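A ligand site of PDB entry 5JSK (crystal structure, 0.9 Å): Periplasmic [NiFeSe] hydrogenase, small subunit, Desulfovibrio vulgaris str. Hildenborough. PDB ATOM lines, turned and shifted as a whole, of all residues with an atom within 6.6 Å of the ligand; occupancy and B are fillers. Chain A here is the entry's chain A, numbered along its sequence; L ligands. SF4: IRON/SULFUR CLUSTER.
FE2 of the ligand is bound by ND1 of His 242. SG of Cys 266 binds FE3 of the ligand, 2.3 Å away. The side-chain sulfur (SG) of Cys 245 is bound to an iron atom (FE4) of the ligand, at 2.3 Å. An iron atom (FE1) of the ligand is bound by the side-chain sulfur of Cys 272. The backbone NH (N) of Arg 267 lies close to a sulfur (S2) of the ligand, 3.4 Å away. The backbone NH (N) of Leu 248 lies close to a sulfur (S1) of the ligand.
The backbone NH (N) of Tyr 268 sits close to the side-chain sulfur (SG) of Cys 266, at 3.3 Å. SD of Met 256 lies close to SG of Cys 266, at 3.7 Å. The side-chain sulfur (SG) of Cys 245 lies close to the backbone NH (N) of Tyr 247 (3.3 Å). N of Cys 272 is in hydrogen-bond range of O of Arg 267, at 3.2 Å. The backbone NH (N) of Gly 274 lies close to the side-chain sulfur (SG) of Cys 272 (3.4 Å). The guanidinium group (NE) of Arg 267 is in hydrogen-bond range of the backbone carbonyl oxygen (O) of Val 294 (2.9 Å). The guanidinium group of Arg 267 sits at hydrogen-bond distance from the side-chain hydroxyl of Tyr 247 (3.4 Å). The guanidinium group (NH1) of Arg 267 sits at hydrogen-bond distance from the backbone carbonyl oxygen (O) of Gly 265 (2.7 Å).
The backbone carbonyl oxygen (O) of Tyr 247 lies close to a sulfur (S1) of the ligand, at 3.6 Å. Ile 241 touches the ligand (CG2 to S3, 3.999 Å). Tyr 251 touches the ligand. Tyr 268 touches the ligand (CB to S4, 3.8 Å). Gly 274 touches the ligand. Pro 275 touches the ligand (CD to S4, 3.8 Å). Val 294 touches the ligand (CG1 to S2, 3.6 Å). Hydrophobic or aromatic side chains that line the ligand: Ile 241, His 242, Tyr 251, Tyr 268, Pro 275 and Val 294. Of the 25 residues printed, 13 come within 4 Å of the ligand. The nearest printed residue that does not touch the ligand is Lys 273 (5.3 Å).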
ATOM      1  N   ILE A 241      18.254  34.176   1.657  1.00  0.00           N
ATOM      2  CA  ILE A 241      19.316  33.772   2.567  1.00  0.00           C
ATOM      3  C   ILE A 241      20.659  33.705   1.856  1.00  0.00           C
ATOM      4  O   ILE A 241      21.654  34.294   2.300  1.00  0.00           O
ATOM      5  CB  ILE A 241      18.978  32.425   3.230  1.00  0.00           C
ATOM      6  CG1 ILE A 241      17.829  32.625   4.207  1.00  0.00           C
ATOM      7  CG2 ILE A 241      20.213  31.837   3.914  1.00  0.00           C
ATOM      8  CD1 ILE A 241      17.458  31.400   4.930  1.00  0.00           C
ATOM      9  N   HIS A 242      20.729  32.954   0.765  1.00  0.00           N
ATOM     10  CA  HIS A 242      22.005  32.665   0.110  1.00  0.00           C
ATOM     11  C   HIS A 242      22.721  33.928  -0.346  1.00  0.00           C
ATOM     12  O   HIS A 242      23.928  34.047  -0.175  1.00  0.00           O
ATOM     13  CB  HIS A 242      21.711  31.742  -1.064  1.00  0.00           C
ATOM     14  CG  HIS A 242      22.862  31.470  -1.975  1.00  0.00           C
ATOM     15  ND1 HIS A 242      23.853  30.560  -1.694  1.00  0.00           N
ATOM     16  CD2 HIS A 242      23.135  31.973  -3.196  1.00  0.00           C
ATOM     17  CE1 HIS A 242      24.707  30.538  -2.697  1.00  0.00           C
ATOM     18  NE2 HIS A 242      24.294  31.374  -3.626  1.00  0.00           N
ATOM     19  N   GLU A 243      21.991  34.876  -0.942  1.00  0.00           N
ATOM     20  CA  GLU A 243      22.638  36.067  -1.461  1.00  0.00           C
ATOM     21  C   GLU A 243      23.212  36.944  -0.357  1.00  0.00           C
ATOM     22  O   GLU A 243      24.002  37.840  -0.646  1.00  0.00           O
ATOM     23  CB  GLU A 243      21.666  36.851  -2.355  1.00  0.00           C
ATOM     24  CG  GLU A 243      21.229  36.097  -3.619  1.00  0.00           C
ATOM     25  CD  GLU A 243      22.380  35.656  -4.527  1.00  0.00           C
ATOM     26  OE1 GLU A 243      23.470  36.273  -4.522  1.00  0.00           O
ATOM     27  OE2 GLU A 243      22.202  34.667  -5.278  1.00  0.00           O
ATOM     28  N   CYS A 245      24.509  35.301   2.563  1.00  0.00           N
ATOM     29  CA  CYS A 245      25.080  34.331   3.464  1.00  0.00           C
ATOM     30  C   CYS A 245      26.571  34.600   3.690  1.00  0.00           C
ATOM     31  O   CYS A 245      27.291  34.914   2.755  1.00  0.00           O
ATOM     32  CB  CYS A 245      24.941  32.940   2.877  1.00  0.00           C
ATOM     33  SG  CYS A 245      25.613  31.623   3.924  1.00  0.00           S
ATOM     34  N   PRO A 246      27.056  34.426   4.931  1.00  0.00           N
ATOM     35  CA  PRO A 246      28.494  34.579   5.182  1.00  0.00           C
ATOM     36  C   PRO A 246      29.378  33.575   4.458  1.00  0.00           C
ATOM     37  O   PRO A 246      30.586  33.823   4.361  1.00  0.00           O
ATOM     38  CB  PRO A 246      28.594  34.439   6.706  1.00  0.00           C
ATOM     39  CG  PRO A 246      27.426  33.693   7.099  1.00  0.00           C
ATOM     40  CD  PRO A 246      26.323  34.099   6.159  1.00  0.00           C
ATOM     41  N   TYR A 247      28.844  32.476   3.942  1.00  0.00           N
ATOM     42  CA  TYR A 247      29.635  31.477   3.238  1.00  0.00           C
ATOM     43  C   TYR A 247      29.522  31.607   1.725  1.00  0.00           C
ATOM     44  O   TYR A 247      30.021  30.749   0.998  1.00  0.00           O
ATOM     45  CB  TYR A 247      29.281  30.054   3.729  1.00  0.00           C
ATOM     46  CG  TYR A 247      29.214  30.020   5.241  1.00  0.00           C
ATOM     47  CD1 TYR A 247      30.331  30.287   6.013  1.00  0.00           C
ATOM     48  CD2 TYR A 247      28.014  29.801   5.888  1.00  0.00           C
ATOM     49  CE1 TYR A 247      30.250  30.318   7.400  1.00  0.00           C
ATOM     50  CE2 TYR A 247      27.925  29.834   7.267  1.00  0.00           C
ATOM     51  CZ  TYR A 247      29.041  30.085   8.023  1.00  0.00           C
ATOM     52  OH  TYR A 247      28.936  30.123   9.405  1.00  0.00           O
ATOM     53  N   LEU A 248      28.931  32.696   1.239  1.00  0.00           N
ATOM     54  CA  LEU A 248      28.702  32.862  -0.195  1.00  0.00           C
ATOM     55  C   LEU A 248      30.005  32.847  -0.982  1.00  0.00           C
ATOM     56  O   LEU A 248      30.049  32.323  -2.108  1.00  0.00           O
ATOM     57  CB  LEU A 248      27.938  34.158  -0.451  1.00  0.00           C
ATOM     58  CG  LEU A 248      27.548  34.472  -1.906  1.00  0.00           C
ATOM     59  CD1 LEU A 248      26.712  33.360  -2.514  1.00  0.00           C
ATOM     60  CD2 LEU A 248      26.822  35.802  -1.965  1.00  0.00           C
ATOM     61  N   ASP A 249      31.080  33.418  -0.436  1.00  0.00           N
ATOM     62  CA  ASP A 249      32.351  33.371  -1.143  1.00  0.00           C
ATOM     63  C   ASP A 249      32.822  31.933  -1.343  1.00  0.00           C
ATOM     64  O   ASP A 249      33.381  31.596  -2.388  1.00  0.00           O
ATOM     65  CB  ASP A 249      33.419  34.173  -0.396  1.00  0.00           C
ATOM     66  CG  ASP A 249      33.200  35.667  -0.484  1.00  0.00           C
ATOM     67  OD1 ASP A 249      32.336  36.123  -1.262  1.00  0.00           O
ATOM     68  OD2 ASP A 249      33.897  36.404   0.241  1.00  0.00           O
ATOM     69  N   LYS A 250      32.606  31.073  -0.346  1.00  0.00           N
ATOM     70  CA  LYS A 250      32.989  29.679  -0.464  1.00  0.00           C
ATOM     71  C   LYS A 250      32.137  28.971  -1.526  1.00  0.00           C
ATOM     72  O   LYS A 250      32.663  28.190  -2.332  1.00  0.00           O
ATOM     73  CB  LYS A 250      32.872  28.968   0.882  1.00  0.00           C
ATOM     74  CG  LYS A 250      33.750  29.566   1.964  1.00  0.00           C
ATOM     75  CD  LYS A 250      35.219  29.485   1.608  1.00  0.00           C
ATOM     76  CE  LYS A 250      36.091  30.091   2.670  1.00  0.00           C
ATOM     77  NZ  LYS A 250      37.487  29.827   2.342  1.00  0.00           N
ATOM     78  N   TYR A 251      30.838  29.237  -1.546  1.00  0.00           N
ATOM     79  CA  TYR A 251      30.000  28.702  -2.609  1.00  0.00           C
ATOM     80  C   TYR A 251      30.553  29.082  -3.976  1.00  0.00           C
ATOM     81  O   TYR A 251      30.723  28.238  -4.861  1.00  0.00           O
ATOM     82  CB  TYR A 251      28.586  29.266  -2.463  1.00  0.00           C
ATOM     83  CG  TYR A 251      27.632  28.873  -3.551  1.00  0.00           C
ATOM     84  CD1 TYR A 251      26.861  27.721  -3.453  1.00  0.00           C
ATOM     85  CD2 TYR A 251      27.489  29.660  -4.697  1.00  0.00           C
ATOM     86  CE1 TYR A 251      25.986  27.369  -4.438  1.00  0.00           C
ATOM     87  CE2 TYR A 251      26.608  29.309  -5.690  1.00  0.00           C
ATOM     88  CZ  TYR A 251      25.854  28.154  -5.554  1.00  0.00           C
ATOM     89  OH  TYR A 251      24.969  27.790  -6.546  1.00  0.00           O
ATOM     90  N   ASP A 252      30.847  30.381  -4.155  1.00  0.00           N
ATOM     91  CA  ASP A 252      31.309  30.849  -5.455  1.00  0.00           C
ATOM     92  C   ASP A 252      32.668  30.269  -5.820  1.00  0.00           C
ATOM     93  O   ASP A 252      32.962  30.120  -7.016  1.00  0.00           O
ATOM     94  CB  ASP A 252      31.315  32.384  -5.482  1.00  0.00           C
ATOM     95  CG  ASP A 252      29.895  32.979  -5.521  1.00  0.00           C
ATOM     96  OD1 ASP A 252      28.963  32.311  -6.001  1.00  0.00           O
ATOM     97  OD2 ASP A 252      29.715  34.131  -5.063  1.00  0.00           O
ATOM     98  N   MET A 256      33.277  23.355  -0.653  1.00  0.00           N
ATOM     99  CA  MET A 256      32.114  22.750  -0.019  1.00  0.00           C
ATOM    100  C   MET A 256      32.550  21.858   1.130  1.00  0.00           C
ATOM    101  O   MET A 256      33.416  21.001   0.964  1.00  0.00           O
ATOM    102  CB  MET A 256      31.390  21.868  -1.034  1.00  0.00           C
ATOM    103  CG  MET A 256      30.896  22.606  -2.220  1.00  0.00           C
ATOM    104  SD  MET A 256      29.581  23.681  -1.668  1.00  0.00           S
ATOM    105  CE  MET A 256      29.288  24.627  -3.168  1.00  0.00           C
ATOM    106  N   GLY A 265      33.678  25.651   4.933  1.00  0.00           N
ATOM    107  CA  GLY A 265      33.125  25.568   3.599  1.00  0.00           C
ATOM    108  C   GLY A 265      31.631  25.895   3.543  1.00  0.00           C
ATOM    109  O   GLY A 265      30.934  25.990   4.552  1.00  0.00           O
ATOM    110  N   CYS A 266      31.162  26.057   2.312  1.00  0.00           N
ATOM    111  CA  CYS A 266      29.732  26.189   2.049  1.00  0.00           C
ATOM    112  C   CYS A 266      29.033  24.847   2.315  1.00  0.00           C
ATOM    113  O   CYS A 266      29.614  23.777   2.165  1.00  0.00           O
ATOM    114  CB  CYS A 266      29.538  26.646   0.606  1.00  0.00           C
ATOM    115  SG  CYS A 266      27.871  26.502  -0.098  1.00  0.00           S
ATOM    116  N   ARG A 267      27.766  24.939   2.731  1.00  0.00           N
ATOM    117  CA  ARG A 267      26.939  23.800   3.112  1.00  0.00           C
ATOM    118  C   ARG A 267      26.097  23.240   1.962  1.00  0.00           C
ATOM    119  O   ARG A 267      25.277  22.350   2.182  1.00  0.00           O
ATOM    120  CB  ARG A 267      26.037  24.196   4.292  1.00  0.00           C
ATOM    121  CG  ARG A 267      26.727  24.373   5.627  1.00  0.00           C
ATOM    122  CD  ARG A 267      27.665  25.574   5.733  1.00  0.00           C
ATOM    123  NE  ARG A 267      27.834  25.932   7.136  1.00  0.00           N
ATOM    124  CZ  ARG A 267      28.892  26.501   7.697  1.00  0.00           C
ATOM    125  NH1 ARG A 267      29.973  26.788   6.984  1.00  0.00           N
ATOM    126  NH2 ARG A 267      28.870  26.775   8.983  1.00  0.00           N
ATOM    127  N   TYR A 268      26.289  23.721   0.730  1.00  0.00           N
ATOM    128  CA  TYR A 268      25.418  23.327  -0.368  1.00  0.00           C
ATOM    129  C   TYR A 268      25.411  21.817  -0.601  1.00  0.00           C
ATOM    130  O   TYR A 268      24.351  21.213  -0.802  1.00  0.00           O
ATOM    131  CB  TYR A 268      25.849  24.062  -1.632  1.00  0.00           C
ATOM    132  CG  TYR A 268      25.000  23.775  -2.824  1.00  0.00           C
ATOM    133  CD1 TYR A 268      23.781  24.402  -2.992  1.00  0.00           C
ATOM    134  CD2 TYR A 268      25.418  22.864  -3.782  1.00  0.00           C
ATOM    135  CE1 TYR A 268      22.999  24.144  -4.089  1.00  0.00           C
ATOM    136  CE2 TYR A 268      24.646  22.596  -4.876  1.00  0.00           C
ATOM    137  CZ  TYR A 268      23.436  23.236  -5.021  1.00  0.00           C
ATOM    138  OH  TYR A 268      22.688  22.945  -6.144  1.00  0.00           O
ATOM    139  N   ASP A 269      26.586  21.173  -0.620  1.00  0.00           N
ATOM    140  CA  ASP A 269      26.631  19.742  -0.899  1.00  0.00           C
ATOM    141  C   ASP A 269      26.017  18.921   0.239  1.00  0.00           C
ATOM    142  O   ASP A 269      25.628  17.771   0.009  1.00  0.00           O
ATOM    143  CB  ASP A 269      28.055  19.267  -1.134  1.00  0.00           C
ATOM    144  CG  ASP A 269      28.613  19.676  -2.484  1.00  0.00           C
ATOM    145  OD1 ASP A 269      27.861  20.170  -3.348  1.00  0.00           O
ATOM    146  OD2 ASP A 269      29.819  19.449  -2.675  1.00  0.00           O
ATOM    147  N   CYS A 272      22.094  22.332   1.875  1.00  0.00           N
ATOM    148  CA  CYS A 272      21.569  23.658   2.200  1.00  0.00           C
ATOM    149  C   CYS A 272      20.596  24.162   1.142  1.00  0.00           C
ATOM    150  O   CYS A 272      20.893  24.173  -0.062  1.00  0.00           O
ATOM    151  CB  CYS A 272      22.729  24.636   2.348  1.00  0.00           C
ATOM    152  SG  CYS A 272      22.202  26.257   2.998  1.00  0.00           S
ATOM    153  N   LYS A 273      19.439  24.652   1.617  1.00  0.00           N
ATOM    154  CA  LYS A 273      18.399  25.221   0.766  1.00  0.00           C
ATOM    155  C   LYS A 273      18.386  26.742   0.795  1.00  0.00           C
ATOM    156  O   LYS A 273      17.442  27.365   0.289  1.00  0.00           O
ATOM    157  CB  LYS A 273      17.017  24.666   1.115  1.00  0.00           C
ATOM    158  CG  LYS A 273      16.939  23.147   1.048  1.00  0.00           C
ATOM    159  CD  LYS A 273      17.439  22.588  -0.274  1.00  0.00           C
ATOM    160  CE  LYS A 273      17.128  21.116  -0.458  1.00  0.00           C
ATOM    161  NZ  LYS A 273      17.682  20.312   0.625  1.00  0.00           N
ATOM    162  N   GLY A 274      19.420  27.370   1.365  1.00  0.00           N
ATOM    163  CA  GLY A 274      19.506  28.816   1.352  1.00  0.00           C
ATOM    164  C   GLY A 274      19.256  29.463   0.007  1.00  0.00           C
ATOM    165  O   GLY A 274      18.606  30.514  -0.062  1.00  0.00           O
ATOM    166  N   PRO A 275      19.754  28.884  -1.090  1.00  0.00           N
ATOM    167  CA  PRO A 275      19.504  29.488  -2.402  1.00  0.00           C
ATOM    168  C   PRO A 275      18.040  29.670  -2.734  1.00  0.00           C
ATOM    169  O   PRO A 275      17.695  30.567  -3.517  1.00  0.00           O
ATOM    170  CB  PRO A 275      20.221  28.536  -3.362  1.00  0.00           C
ATOM    171  CG  PRO A 275      21.336  27.980  -2.554  1.00  0.00           C
ATOM    172  CD  PRO A 275      20.734  27.784  -1.182  1.00  0.00           C
ATOM    173  N   TRP A 292      22.266  29.902  14.156  1.00  0.00           N
ATOM    174  CA  TRP A 292      21.232  29.778  13.138  1.00  0.00           C
ATOM    175  C   TRP A 292      21.515  28.529  12.317  1.00  0.00           C
ATOM    176  O   TRP A 292      22.576  27.922  12.418  1.00  0.00           O
ATOM    177  CB  TRP A 292      21.087  31.003  12.252  1.00  0.00           C
ATOM    178  CG  TRP A 292      22.232  31.315  11.341  1.00  0.00           C
ATOM    179  CD1 TRP A 292      23.527  31.564  11.697  1.00  0.00           C
ATOM    180  CD2 TRP A 292      22.151  31.498   9.923  1.00  0.00           C
ATOM    181  NE1 TRP A 292      24.256  31.882  10.569  1.00  0.00           N
ATOM    182  CE2 TRP A 292      23.437  31.848   9.477  1.00  0.00           C
ATOM    183  CE3 TRP A 292      21.120  31.376   8.987  1.00  0.00           C
ATOM    184  CZ2 TRP A 292      23.715  32.093   8.121  1.00  0.00           C
ATOM    185  CZ3 TRP A 292      21.390  31.640   7.657  1.00  0.00           C
ATOM    186  CH2 TRP A 292      22.681  31.990   7.235  1.00  0.00           C
ATOM    187  N   VAL A 294      22.166  27.629   9.201  1.00  0.00           N
ATOM    188  CA  VAL A 294      23.261  27.475   8.259  1.00  0.00           C
ATOM    189  C   VAL A 294      24.592  27.370   8.992  1.00  0.00           C
ATOM    190  O   VAL A 294      25.454  26.585   8.608  1.00  0.00           O
ATOM    191  CB  VAL A 294      23.242  28.606   7.213  1.00  0.00           C
ATOM    192  CG1 VAL A 294      24.477  28.562   6.331  1.00  0.00           C
ATOM    193  CG2 VAL A 294      21.996  28.534   6.357  1.00  0.00           C
ATOM    194  N   ALA A 297      24.226  23.673  10.800  1.00  0.00           N
ATOM    195  CA  ALA A 297      23.941  22.512   9.971  1.00  0.00           C
ATOM    196  C   ALA A 297      23.633  22.996   8.561  1.00  0.00           C
ATOM    197  O   ALA A 297      24.546  23.441   7.850  1.00  0.00           O
ATOM    198  CB  ALA A 297      22.840  21.653  10.584  1.00  0.00           C
ATOM    199  N   CYS A 299      20.254  25.038   6.085  1.00  0.00           N
ATOM    200  CA  CYS A 299      18.893  25.522   5.937  1.00  0.00           C
ATOM    201  C   CYS A 299      18.059  24.457   5.225  1.00  0.00           C
ATOM    202  O   CYS A 299      18.503  23.861   4.232  1.00  0.00           O
ATOM    203  CB  CYS A 299      18.886  26.845   5.151  1.00  0.00           C
ATOM    204  SG  CYS A 299      17.253  27.543   4.736  1.00  0.00           S
HETATM  205 FE1  SF4 L   1      23.806  27.649   2.036  1.00  0.00          FE
HETATM  206 FE2  SF4 L   1      24.281  29.459   0.034  1.00  0.00          FE
HETATM  207 FE3  SF4 L   1      26.335  27.902   0.871  1.00  0.00          FE
HETATM  208 FE4  SF4 L   1      25.304  29.867   2.457  1.00  0.00          FE
HETATM  209  S1  SF4 L   1      26.463  30.145   0.508  1.00  0.00           S
HETATM  210  S2  SF4 L   1      25.886  27.743   3.120  1.00  0.00           S
HETATM  211  S3  SF4 L   1      23.036  29.814   1.932  1.00  0.00           S
HETATM  212  S4  SF4 L   1      24.355  27.171  -0.148  1.00  0.00           S
